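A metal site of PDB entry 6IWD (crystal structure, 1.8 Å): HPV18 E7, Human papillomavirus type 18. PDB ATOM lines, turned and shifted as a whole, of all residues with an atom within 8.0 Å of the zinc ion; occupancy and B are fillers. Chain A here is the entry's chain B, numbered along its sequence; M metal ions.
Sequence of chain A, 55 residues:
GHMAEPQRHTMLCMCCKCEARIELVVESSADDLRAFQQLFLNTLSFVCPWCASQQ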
ATOM      1  N   MET A  14     -20.544  11.442 -21.294  1.00  0.00           N
ATOM      2  CA  MET A  14     -20.431  11.437 -19.849  1.00  0.00           C
ATOM      3  C   MET A  14     -19.928  12.788 -19.367  1.00  0.00           C
ATOM      4  O   MET A  14     -19.041  13.383 -19.986  1.00  0.00           O
ATOM      5  CB  MET A  14     -19.490  10.313 -19.393  1.00  0.00           C
ATOM      6  CG  MET A  14     -19.478  10.045 -17.891  1.00  0.00           C
ATOM      7  SD  MET A  14     -18.123   8.949 -17.341  1.00  0.00           S
ATOM      8  CE  MET A  14     -16.697   9.927 -17.815  1.00  0.00           C
ATOM      9  N   CYS A  15     -20.502  13.286 -18.282  1.00  0.00           N
ATOM     10  CA  CYS A  15     -19.957  14.482 -17.647  1.00  0.00           C
ATOM     11  C   CYS A  15     -18.510  14.221 -17.220  1.00  0.00           C
ATOM     12  O   CYS A  15     -18.192  13.169 -16.658  1.00  0.00           O
ATOM     13  CB  CYS A  15     -20.794  14.896 -16.441  1.00  0.00           C
ATOM     14  SG  CYS A  15     -20.069  16.277 -15.521  1.00  0.00           S
ATOM     15  N   CYS A  16     -17.642  15.196 -17.483  1.00  0.00           N
ATOM     16  CA  CYS A  16     -16.239  15.017 -17.139  1.00  0.00           C
ATOM     17  C   CYS A  16     -15.966  15.238 -15.651  1.00  0.00           C
ATOM     18  O   CYS A  16     -14.806  15.124 -15.238  1.00  0.00           O
ATOM     19  CB  CYS A  16     -15.357  15.937 -17.973  1.00  0.00           C
ATOM     20  SG  CYS A  16     -15.698  17.703 -17.795  1.00  0.00           S
ATOM     21  N   LYS A  17     -16.996  15.528 -14.854  1.00  0.00           N
ATOM     22  CA  LYS A  17     -16.817  15.745 -13.429  1.00  0.00           C
ATOM     23  C   LYS A  17     -17.478  14.703 -12.548  1.00  0.00           C
ATOM     24  O   LYS A  17     -17.021  14.488 -11.422  1.00  0.00           O
ATOM     25  CB  LYS A  17     -17.330  17.130 -13.026  1.00  0.00           C
ATOM     26  CG  LYS A  17     -16.600  18.280 -13.673  1.00  0.00           C
ATOM     27  CD  LYS A  17     -15.107  18.210 -13.382  1.00  0.00           C
ATOM     28  CE  LYS A  17     -14.300  18.607 -14.607  1.00  0.00           C
ATOM     29  NZ  LYS A  17     -13.075  17.757 -14.782  1.00  0.00           N
ATOM     30  N   CYS A  18     -18.549  14.035 -13.012  1.00  0.00           N
ATOM     31  CA  CYS A  18     -19.374  13.270 -12.095  1.00  0.00           C
ATOM     32  C   CYS A  18     -19.952  11.978 -12.650  1.00  0.00           C
ATOM     33  O   CYS A  18     -20.815  11.372 -11.994  1.00  0.00           O
ATOM     34  CB  CYS A  18     -20.525  14.121 -11.585  1.00  0.00           C
ATOM     35  SG  CYS A  18     -21.926  14.138 -12.718  1.00  0.00           S
ATOM     36  N   GLU A  19     -19.547  11.540 -13.844  1.00  0.00           N
ATOM     37  CA  GLU A  19     -19.955  10.252 -14.415  1.00  0.00           C
ATOM     38  C   GLU A  19     -21.415  10.220 -14.868  1.00  0.00           C
ATOM     39  O   GLU A  19     -21.857   9.205 -15.431  1.00  0.00           O
ATOM     40  CB  GLU A  19     -19.708   9.090 -13.434  1.00  0.00           C
ATOM     41  CG  GLU A  19     -19.097   7.825 -14.021  1.00  0.00           C
ATOM     42  CD  GLU A  19     -18.549   6.912 -12.930  1.00  0.00           C
ATOM     43  OE1 GLU A  19     -18.858   5.696 -12.934  1.00  0.00           O
ATOM     44  OE2 GLU A  19     -17.805   7.408 -12.059  1.00  0.00           O
ATOM     45  N   ALA A  20     -22.204  11.270 -14.634  1.00  0.00           N
ATOM     46  CA  ALA A  20     -23.577  11.269 -15.114  1.00  0.00           C
ATOM     47  C   ALA A  20     -23.602  11.336 -16.641  1.00  0.00           C
ATOM     48  O   ALA A  20     -22.731  11.937 -17.275  1.00  0.00           O
ATOM     49  CB  ALA A  20     -24.361  12.443 -14.541  1.00  0.00           C
ATOM     50  N   ARG A  21     -24.615  10.688 -17.230  1.00  0.00           N
ATOM     51  CA  ARG A  21     -24.779  10.697 -18.668  1.00  0.00           C
ATOM     52  C   ARG A  21     -25.431  11.987 -19.137  1.00  0.00           C
ATOM     53  O   ARG A  21     -26.378  12.499 -18.511  1.00  0.00           O
ATOM     54  CB  ARG A  21     -25.626   9.501 -19.123  1.00  0.00           C
ATOM     55  CG  ARG A  21     -24.979   8.159 -18.854  1.00  0.00           C
ATOM     56  CD  ARG A  21     -26.029   7.080 -18.753  1.00  0.00           C
ATOM     57  NE  ARG A  21     -26.731   6.898 -20.016  1.00  0.00           N
ATOM     58  CZ  ARG A  21     -26.527   5.870 -20.845  1.00  0.00           C
ATOM     59  NH1 ARG A  21     -25.627   4.944 -20.527  1.00  0.00           N
ATOM     60  NH2 ARG A  21     -27.219   5.783 -21.973  1.00  0.00           N
ATOM     61  N   ILE A  22     -24.943  12.525 -20.254  1.00  0.00           N
ATOM     62  CA  ILE A  22     -25.452  13.748 -20.835  1.00  0.00           C
ATOM     63  C   ILE A  22     -26.020  13.418 -22.205  1.00  0.00           C
ATOM     64  O   ILE A  22     -25.356  12.752 -23.006  1.00  0.00           O
ATOM     65  CB  ILE A  22     -24.367  14.832 -20.943  1.00  0.00           C
ATOM     66  CG1 ILE A  22     -23.840  15.200 -19.557  1.00  0.00           C
ATOM     67  CG2 ILE A  22     -24.887  16.047 -21.702  1.00  0.00           C
ATOM     68  CD1 ILE A  22     -22.644  16.127 -19.600  1.00  0.00           C
ATOM     69  N   PHE A  46     -18.092  17.626 -21.908  1.00  0.00           N
ATOM     70  CA  PHE A  46     -19.186  18.428 -21.383  1.00  0.00           C
ATOM     71  C   PHE A  46     -19.333  18.258 -19.881  1.00  0.00           C
ATOM     72  O   PHE A  46     -19.015  17.207 -19.319  1.00  0.00           O
ATOM     73  CB  PHE A  46     -20.498  18.075 -22.080  1.00  0.00           C
ATOM     74  CG  PHE A  46     -20.611  18.666 -23.445  1.00  0.00           C
ATOM     75  CD1 PHE A  46     -19.940  18.093 -24.518  1.00  0.00           C
ATOM     76  CD2 PHE A  46     -21.337  19.831 -23.651  1.00  0.00           C
ATOM     77  CE1 PHE A  46     -20.019  18.664 -25.780  1.00  0.00           C
ATOM     78  CE2 PHE A  46     -21.430  20.400 -24.912  1.00  0.00           C
ATOM     79  CZ  PHE A  46     -20.771  19.815 -25.984  1.00  0.00           C
ATOM     80  N   VAL A  47     -19.790  19.321 -19.229  1.00  0.00           N
ATOM     81  CA  VAL A  47     -20.070  19.355 -17.801  1.00  0.00           C
ATOM     82  C   VAL A  47     -21.577  19.374 -17.618  1.00  0.00           C
ATOM     83  O   VAL A  47     -22.264  20.206 -18.231  1.00  0.00           O
ATOM     84  CB  VAL A  47     -19.421  20.582 -17.136  1.00  0.00           C
ATOM     85  CG1 VAL A  47     -19.646  20.553 -15.642  1.00  0.00           C
ATOM     86  CG2 VAL A  47     -17.933  20.661 -17.463  1.00  0.00           C
ATOM     87  N   CYS A  48     -22.095  18.458 -16.794  1.00  0.00           N
ATOM     88  CA  CYS A  48     -23.531  18.389 -16.583  1.00  0.00           C
ATOM     89  C   CYS A  48     -24.015  19.642 -15.873  1.00  0.00           C
ATOM     90  O   CYS A  48     -23.215  20.412 -15.338  1.00  0.00           O
ATOM     91  CB  CYS A  48     -23.896  17.122 -15.805  1.00  0.00           C
ATOM     92  SG  CYS A  48     -23.495  17.068 -14.038  1.00  0.00           S
ATOM     93  N   PRO A  49     -25.325  19.924 -15.904  1.00  0.00           N
ATOM     94  CA  PRO A  49     -25.803  21.164 -15.285  1.00  0.00           C
ATOM     95  C   PRO A  49     -25.510  21.254 -13.805  1.00  0.00           C
ATOM     96  O   PRO A  49     -25.151  22.328 -13.308  1.00  0.00           O
ATOM     97  CB  PRO A  49     -27.315  21.130 -15.566  1.00  0.00           C
ATOM     98  CG  PRO A  49     -27.431  20.336 -16.816  1.00  0.00           C
ATOM     99  CD  PRO A  49     -26.391  19.259 -16.683  1.00  0.00           C
ATOM    100  N   TRP A  50     -25.614  20.141 -13.081  1.00  0.00           N
ATOM    101  CA  TRP A  50     -25.365  20.177 -11.642  1.00  0.00           C
ATOM    102  C   TRP A  50     -23.921  20.571 -11.345  1.00  0.00           C
ATOM    103  O   TRP A  50     -23.669  21.507 -10.576  1.00  0.00           O
ATOM    104  CB  TRP A  50     -25.695  18.845 -10.983  1.00  0.00           C
ATOM    105  CG  TRP A  50     -25.649  18.960  -9.491  1.00  0.00           C
ATOM    106  CD1 TRP A  50     -26.699  19.240  -8.671  1.00  0.00           C
ATOM    107  CD2 TRP A  50     -24.489  18.869  -8.660  1.00  0.00           C
ATOM    108  NE1 TRP A  50     -26.272  19.313  -7.368  1.00  0.00           N
ATOM    109  CE2 TRP A  50     -24.914  19.090  -7.333  1.00  0.00           C
ATOM    110  CE3 TRP A  50     -23.135  18.625  -8.893  1.00  0.00           C
ATOM    111  CZ2 TRP A  50     -24.049  19.063  -6.259  1.00  0.00           C
ATOM    112  CZ3 TRP A  50     -22.279  18.605  -7.828  1.00  0.00           C
ATOM    113  CH2 TRP A  50     -22.732  18.819  -6.514  1.00  0.00           C
ATOM    114  N   CYS A  51     -22.960  19.878 -11.958  1.00  0.00           N
ATOM    115  CA  CYS A  51     -21.547  20.221 -11.760  1.00  0.00           C
ATOM    116  C   CYS A  51     -21.229  21.620 -12.236  1.00  0.00           C
ATOM    117  O   CYS A  51     -20.240  22.213 -11.782  1.00  0.00           O
ATOM    118  CB  CYS A  51     -20.657  19.214 -12.481  1.00  0.00           C
ATOM    119  SG  CYS A  51     -20.712  17.586 -11.764  1.00  0.00           S
ATOM    120  N   ALA A  52     -22.031  22.162 -13.154  1.00  0.00           N
ATOM    121  CA  ALA A  52     -21.807  23.527 -13.624  1.00  0.00           C
ATOM    122  C   ALA A  52     -22.170  24.564 -12.574  1.00  0.00           C
ATOM    123  O   ALA A  52     -21.599  25.660 -12.554  1.00  0.00           O
ATOM    124  CB  ALA A  52     -22.602  23.768 -14.910  1.00  0.00           C
HETATM  125 ZN    ZN M   1     -21.584  16.223 -13.480  1.00  0.00          ZN
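The backbone NH (N) of Lys 17 sits close to the side-chain sulfur (SG) of Cys 15. The backbone carbonyl oxygen (O) of Ala 20 lies within hydrogen-bond range of the backbone NH (N) of Cys 15 (2.8 Å). The side-chain sulfur (SG) of Cys 18 sits close to the backbone NH (N) of Ala 20, 3.5 Å away.
Four residues have an atom within 4 Å of the zinc ion: Cys 15, Cys 18, Cys 48 and Cys 51.
The zinc ion is bound by SG of Cys 48 (2.2 Å), SG of Cys 18 (2.2 Å), SG of Cys 51 (2.4 Å) and SG of Cys 15 (2.5 Å).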
